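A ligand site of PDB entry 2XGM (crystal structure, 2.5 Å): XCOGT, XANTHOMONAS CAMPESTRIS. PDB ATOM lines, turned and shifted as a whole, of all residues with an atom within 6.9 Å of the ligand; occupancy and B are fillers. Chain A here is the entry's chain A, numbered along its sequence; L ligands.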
ATOM      1  N   ALA A 217       6.836 -30.940  -8.164  1.00  0.00           N
ATOM      2  CA  ALA A 217       7.525 -30.067  -7.205  1.00  0.00           C
ATOM      3  C   ALA A 217       6.645 -28.905  -6.745  1.00  0.00           C
ATOM      4  O   ALA A 217       7.035 -27.708  -6.874  1.00  0.00           O
ATOM      5  CB  ALA A 217       8.861 -29.585  -7.755  1.00  0.00           C
ATOM      6  N   PRO A 219       3.048 -27.742  -3.938  1.00  0.00           N
ATOM      7  CA  PRO A 219       2.474 -28.220  -2.670  1.00  0.00           C
ATOM      8  C   PRO A 219       1.806 -29.639  -2.667  1.00  0.00           C
ATOM      9  O   PRO A 219       2.235 -30.517  -1.891  1.00  0.00           O
ATOM     10  CB  PRO A 219       1.501 -27.099  -2.296  1.00  0.00           C
ATOM     11  CG  PRO A 219       2.307 -25.789  -2.795  1.00  0.00           C
ATOM     12  CD  PRO A 219       2.971 -26.265  -4.096  1.00  0.00           C
ATOM     13  N   LEU A 222       3.790 -32.674  -3.085  1.00  0.00           N
ATOM     14  CA  LEU A 222       4.769 -32.515  -2.030  1.00  0.00           C
ATOM     15  C   LEU A 222       4.218 -32.886  -0.686  1.00  0.00           C
ATOM     16  O   LEU A 222       4.990 -33.177   0.204  1.00  0.00           O
ATOM     17  CB  LEU A 222       5.287 -31.051  -1.995  1.00  0.00           C
ATOM     18  CG  LEU A 222       6.172 -30.532  -0.842  1.00  0.00           C
ATOM     19  CD1 LEU A 222       7.368 -31.505  -0.399  1.00  0.00           C
ATOM     20  CD2 LEU A 222       6.696 -29.135  -1.146  1.00  0.00           C
ATOM     21  N   PHE A 383       7.689 -17.962   6.392  1.00  0.00           N
ATOM     22  CA  PHE A 383       7.696 -18.279   5.005  1.00  0.00           C
ATOM     23  C   PHE A 383       6.256 -18.578   4.594  1.00  0.00           C
ATOM     24  O   PHE A 383       5.688 -19.600   4.977  1.00  0.00           O
ATOM     25  CB  PHE A 383       8.589 -19.483   4.686  1.00  0.00           C
ATOM     26  CG  PHE A 383      10.049 -19.316   5.075  1.00  0.00           C
ATOM     27  CD1 PHE A 383      10.667 -18.072   5.055  1.00  0.00           C
ATOM     28  CD2 PHE A 383      10.784 -20.431   5.430  1.00  0.00           C
ATOM     29  CE1 PHE A 383      11.990 -17.921   5.398  1.00  0.00           C
ATOM     30  CE2 PHE A 383      12.133 -20.313   5.801  1.00  0.00           C
ATOM     31  CZ  PHE A 383      12.740 -19.038   5.778  1.00  0.00           C
ATOM     32  N   ASN A 384       5.662 -17.703   3.802  1.00  0.00           N
ATOM     33  CA  ASN A 384       4.277 -17.858   3.438  1.00  0.00           C
ATOM     34  C   ASN A 384       3.993 -17.111   2.161  1.00  0.00           C
ATOM     35  O   ASN A 384       4.845 -16.409   1.693  1.00  0.00           O
ATOM     36  CB  ASN A 384       3.424 -17.280   4.535  1.00  0.00           C
ATOM     37  CG  ASN A 384       2.476 -18.274   5.064  1.00  0.00           C
ATOM     38  OD1 ASN A 384       2.309 -19.356   4.495  1.00  0.00           O
ATOM     39  ND2 ASN A 384       1.824 -17.928   6.159  1.00  0.00           N
ATOM     40  N   ASN A 385       2.810 -17.254   1.589  1.00  0.00           N
ATOM     41  CA  ASN A 385       2.531 -16.598   0.371  1.00  0.00           C
ATOM     42  C   ASN A 385       2.377 -15.078   0.665  1.00  0.00           C
ATOM     43  O   ASN A 385       1.736 -14.701   1.661  1.00  0.00           O
ATOM     44  CB  ASN A 385       1.261 -17.215  -0.194  1.00  0.00           C
ATOM     45  CG  ASN A 385       1.363 -18.791  -0.412  1.00  0.00           C
ATOM     46  OD1 ASN A 385       1.609 -19.266  -1.547  1.00  0.00           O
ATOM     47  ND2 ASN A 385       1.201 -19.571   0.670  1.00  0.00           N
ATOM     48  N   LEU A 412       9.978 -14.801   2.980  1.00  0.00           N
ATOM     49  CA  LEU A 412      10.152 -15.155   1.545  1.00  0.00           C
ATOM     50  C   LEU A 412      10.140 -13.888   0.750  1.00  0.00           C
ATOM     51  O   LEU A 412       9.320 -12.992   0.988  1.00  0.00           O
ATOM     52  CB  LEU A 412       9.052 -16.061   1.030  1.00  0.00           C
ATOM     53  CG  LEU A 412       9.123 -17.492   1.585  1.00  0.00           C
ATOM     54  CD1 LEU A 412       8.064 -18.401   0.949  1.00  0.00           C
ATOM     55  CD2 LEU A 412      10.501 -18.064   1.355  1.00  0.00           C
ATOM     56  N   SER A 413      11.074 -13.782  -0.191  1.00  0.00           N
ATOM     57  CA  SER A 413      11.108 -12.630  -1.082  1.00  0.00           C
ATOM     58  C   SER A 413       9.820 -12.649  -1.898  1.00  0.00           C
ATOM     59  O   SER A 413       9.480 -13.662  -2.507  1.00  0.00           O
ATOM     60  CB  SER A 413      12.288 -12.731  -2.016  1.00  0.00           C
ATOM     61  OG  SER A 413      12.482 -11.507  -2.647  1.00  0.00           O
ATOM     62  N   MET A 439      14.283 -14.346   1.743  1.00  0.00           N
ATOM     63  CA  MET A 439      14.853 -15.534   1.097  1.00  0.00           C
ATOM     64  C   MET A 439      14.484 -15.549  -0.387  1.00  0.00           C
ATOM     65  O   MET A 439      13.327 -15.285  -0.755  1.00  0.00           O
ATOM     66  CB  MET A 439      14.391 -16.801   1.797  1.00  0.00           C
ATOM     67  CG  MET A 439      15.027 -18.056   1.210  1.00  0.00           C
ATOM     68  SD  MET A 439      14.508 -19.620   1.960  1.00  0.00           S
ATOM     69  CE  MET A 439      13.314 -20.218   0.818  1.00  0.00           C
ATOM     70  N   PRO A 440      15.441 -15.849  -1.268  1.00  0.00           N
ATOM     71  CA  PRO A 440      15.032 -15.932  -2.673  1.00  0.00           C
ATOM     72  C   PRO A 440      14.310 -17.271  -2.973  1.00  0.00           C
ATOM     73  O   PRO A 440      14.096 -18.084  -2.062  1.00  0.00           O
ATOM     74  CB  PRO A 440      16.349 -15.827  -3.440  1.00  0.00           C
ATOM     75  CG  PRO A 440      17.390 -16.388  -2.478  1.00  0.00           C
ATOM     76  CD  PRO A 440      16.834 -16.296  -1.061  1.00  0.00           C
ATOM     77  N   LYS A 441      13.915 -17.458  -4.228  1.00  0.00           N
ATOM     78  CA  LYS A 441      13.198 -18.666  -4.652  1.00  0.00           C
ATOM     79  C   LYS A 441      14.254 -19.759  -4.733  1.00  0.00           C
ATOM     80  O   LYS A 441      15.357 -19.495  -5.224  1.00  0.00           O
ATOM     81  CB  LYS A 441      12.559 -18.464  -6.033  1.00  0.00           C
ATOM     82  CG  LYS A 441      11.238 -19.240  -6.259  1.00  0.00           C
ATOM     83  CD  LYS A 441      11.019 -19.613  -7.770  1.00  0.00           C
ATOM     84  CE  LYS A 441       9.717 -20.482  -7.896  1.00  0.00           C
ATOM     85  NZ  LYS A 441       9.640 -21.563  -6.784  1.00  0.00           N
ATOM     86  N   LEU A 442      13.963 -20.961  -4.240  1.00  0.00           N
ATOM     87  CA  LEU A 442      14.955 -22.019  -4.219  1.00  0.00           C
ATOM     88  C   LEU A 442      14.300 -23.398  -4.351  1.00  0.00           C
ATOM     89  O   LEU A 442      13.181 -23.599  -3.857  1.00  0.00           O
ATOM     90  CB  LEU A 442      15.722 -21.972  -2.899  1.00  0.00           C
ATOM     91  CG  LEU A 442      16.714 -20.851  -2.607  1.00  0.00           C
ATOM     92  CD1 LEU A 442      17.069 -20.975  -1.125  1.00  0.00           C
ATOM     93  CD2 LEU A 442      17.943 -20.928  -3.487  1.00  0.00           C
ATOM     94  N   PRO A 443      14.999 -24.327  -5.000  1.00  0.00           N
ATOM     95  CA  PRO A 443      14.508 -25.684  -5.009  1.00  0.00           C
ATOM     96  C   PRO A 443      14.127 -26.153  -3.625  1.00  0.00           C
ATOM     97  O   PRO A 443      14.770 -25.798  -2.641  1.00  0.00           O
ATOM     98  CB  PRO A 443      15.699 -26.464  -5.540  1.00  0.00           C
ATOM     99  CG  PRO A 443      16.351 -25.475  -6.499  1.00  0.00           C
ATOM    100  CD  PRO A 443      16.215 -24.162  -5.806  1.00  0.00           C
ATOM    101  N   HIS A 444      13.073 -26.960  -3.536  1.00  0.00           N
ATOM    102  CA  HIS A 444      12.620 -27.441  -2.226  1.00  0.00           C
ATOM    103  C   HIS A 444      13.789 -27.833  -1.331  1.00  0.00           C
ATOM    104  O   HIS A 444      13.884 -27.322  -0.206  1.00  0.00           O
ATOM    105  CB  HIS A 444      11.548 -28.567  -2.268  1.00  0.00           C
ATOM    106  CG  HIS A 444      10.949 -28.842  -0.921  1.00  0.00           C
ATOM    107  ND1 HIS A 444      10.006 -28.017  -0.341  1.00  0.00           N
ATOM    108  CD2 HIS A 444      11.226 -29.806   0.002  1.00  0.00           C
ATOM    109  CE1 HIS A 444       9.715 -28.463   0.882  1.00  0.00           C
ATOM    110  NE2 HIS A 444      10.445 -29.547   1.112  1.00  0.00           N
ATOM    111  N   PRO A 445      14.686 -28.724  -1.805  1.00  0.00           N
ATOM    112  CA  PRO A 445      15.648 -29.256  -0.840  1.00  0.00           C
ATOM    113  C   PRO A 445      16.505 -28.196  -0.208  1.00  0.00           C
ATOM    114  O   PRO A 445      16.818 -28.291   0.959  1.00  0.00           O
ATOM    115  CB  PRO A 445      16.509 -30.210  -1.662  1.00  0.00           C
ATOM    116  CG  PRO A 445      15.659 -30.593  -2.779  1.00  0.00           C
ATOM    117  CD  PRO A 445      14.858 -29.340  -3.129  1.00  0.00           C
ATOM    118  N   TYR A 447      15.635 -24.860  -0.062  1.00  0.00           N
ATOM    119  CA  TYR A 447      14.657 -24.155   0.744  1.00  0.00           C
ATOM    120  C   TYR A 447      14.385 -24.886   2.076  1.00  0.00           C
ATOM    121  O   TYR A 447      14.499 -24.307   3.182  1.00  0.00           O
ATOM    122  CB  TYR A 447      13.370 -24.004  -0.059  1.00  0.00           C
ATOM    123  CG  TYR A 447      12.138 -23.987   0.806  1.00  0.00           C
ATOM    124  CD1 TYR A 447      11.763 -22.820   1.483  1.00  0.00           C
ATOM    125  CD2 TYR A 447      11.345 -25.144   0.966  1.00  0.00           C
ATOM    126  CE1 TYR A 447      10.632 -22.793   2.298  1.00  0.00           C
ATOM    127  CE2 TYR A 447      10.212 -25.127   1.781  1.00  0.00           C
ATOM    128  CZ  TYR A 447       9.867 -23.943   2.464  1.00  0.00           C
ATOM    129  OH  TYR A 447       8.752 -23.908   3.305  1.00  0.00           O
ATOM    130  N   LEU A 448      14.038 -26.177   2.005  1.00  0.00           N
ATOM    131  CA  LEU A 448      13.732 -26.883   3.242  1.00  0.00           C
ATOM    132  C   LEU A 448      14.887 -26.762   4.207  1.00  0.00           C
ATOM    133  O   LEU A 448      14.664 -26.692   5.403  1.00  0.00           O
ATOM    134  CB  LEU A 448      13.330 -28.327   2.994  1.00  0.00           C
ATOM    135  CG  LEU A 448      12.832 -29.004   4.282  1.00  0.00           C
ATOM    136  CD1 LEU A 448      11.555 -28.356   4.810  1.00  0.00           C
ATOM    137  CD2 LEU A 448      12.698 -30.567   4.176  1.00  0.00           C
ATOM    138  N   TYR A 451      15.159 -23.868   7.222  1.00  0.00           N
ATOM    139  CA  TYR A 451      14.490 -23.935   8.521  1.00  0.00           C
ATOM    140  C   TYR A 451      15.395 -24.313   9.711  1.00  0.00           C
ATOM    141  O   TYR A 451      15.040 -24.098  10.882  1.00  0.00           O
ATOM    142  CB  TYR A 451      13.327 -24.920   8.464  1.00  0.00           C
ATOM    143  CG  TYR A 451      12.116 -24.415   7.711  1.00  0.00           C
ATOM    144  CD1 TYR A 451      11.859 -24.856   6.432  1.00  0.00           C
ATOM    145  CD2 TYR A 451      11.241 -23.497   8.291  1.00  0.00           C
ATOM    146  CE1 TYR A 451      10.768 -24.394   5.743  1.00  0.00           C
ATOM    147  CE2 TYR A 451      10.130 -23.012   7.604  1.00  0.00           C
ATOM    148  CZ  TYR A 451       9.912 -23.478   6.334  1.00  0.00           C
ATOM    149  OH  TYR A 451       8.824 -23.016   5.631  1.00  0.00           O
ATOM    150  N   THR A 467       1.373 -25.707   3.808  1.00  0.00           N
ATOM    151  CA  THR A 467       2.569 -26.521   3.590  1.00  0.00           C
ATOM    152  C   THR A 467       3.802 -25.983   4.314  1.00  0.00           C
ATOM    153  O   THR A 467       4.651 -26.779   4.763  1.00  0.00           O
ATOM    154  CB  THR A 467       2.973 -26.667   2.110  1.00  0.00           C
ATOM    155  OG1 THR A 467       2.813 -25.416   1.442  1.00  0.00           O
ATOM    156  CG2 THR A 467       2.082 -27.583   1.439  1.00  0.00           C
ATOM    157  N   THR A 468       3.918 -24.649   4.425  1.00  0.00           N
ATOM    158  CA  THR A 468       5.101 -24.145   5.095  1.00  0.00           C
ATOM    159  C   THR A 468       5.044 -24.417   6.587  1.00  0.00           C
ATOM    160  O   THR A 468       6.094 -24.674   7.235  1.00  0.00           O
ATOM    161  CB  THR A 468       5.355 -22.700   4.845  1.00  0.00           C
ATOM    162  OG1 THR A 468       4.226 -21.956   5.275  1.00  0.00           O
ATOM    163  CG2 THR A 468       5.589 -22.457   3.394  1.00  0.00           C
ATOM    164  N   ASP A 471       6.293 -27.938   6.899  1.00  0.00           N
ATOM    165  CA  ASP A 471       7.714 -27.920   6.592  1.00  0.00           C
ATOM    166  C   ASP A 471       8.500 -27.532   7.796  1.00  0.00           C
ATOM    167  O   ASP A 471       9.436 -28.215   8.140  1.00  0.00           O
ATOM    168  CB  ASP A 471       8.022 -26.923   5.482  1.00  0.00           C
ATOM    169  CG  ASP A 471       7.577 -27.405   4.117  1.00  0.00           C
ATOM    170  OD1 ASP A 471       7.236 -28.625   3.989  1.00  0.00           O
ATOM    171  OD2 ASP A 471       7.567 -26.549   3.183  1.00  0.00           O
HETATM  172  O1  LIG L   1       7.347 -21.921  -0.440  1.00  0.00           O
HETATM  173  C1  LIG L   1       8.283 -22.352  -1.129  1.00  0.00           C
HETATM  174  C2  LIG L   1       9.191 -21.503  -1.773  1.00  0.00           C
HETATM  175  O2  LIG L   1       9.097 -20.288  -1.694  1.00  0.00           O
HETATM  176  C3  LIG L   1      10.233 -22.034  -2.523  1.00  0.00           C
HETATM  177  O3  LIG L   1      11.052 -21.298  -3.086  1.00  0.00           O
HETATM  178  N1  LIG L   1      10.374 -23.425  -2.634  1.00  0.00           N
HETATM  179  C4  LIG L   1       9.458 -24.273  -1.984  1.00  0.00           C
HETATM  180  O4  LIG L   1       9.568 -25.489  -2.074  1.00  0.00           O
HETATM  181  N2  LIG L   1       8.424 -23.742  -1.239  1.00  0.00           N
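O3 of the ligand sits at hydrogen-bond distance from N of Leu 442, 3.1 Å away. The backbone carbonyl oxygen of Leu 442 is in hydrogen-bond range of a nitrogen (N1) of the ligand (3.1 Å). ND1 of His 444 lies within hydrogen-bond range of O4 of the ligand (3.1 Å).
OD2 of Asp 471 lies within hydrogen-bond range of OH of Tyr 447, 2.9 Å away. The side-chain hydroxyl (OH) of Tyr 447 sits at hydrogen-bond distance from the side-chain hydroxyl (OH) of Tyr 451, at 2.5 Å.
CD1 of Leu 412 touches O2 of the ligand (3.4 Å). Lys 441 touches the ligand (CA to O3, 3.7 Å). Tyr 447 touches the ligand (CD2 to O4, 3.5 Å).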
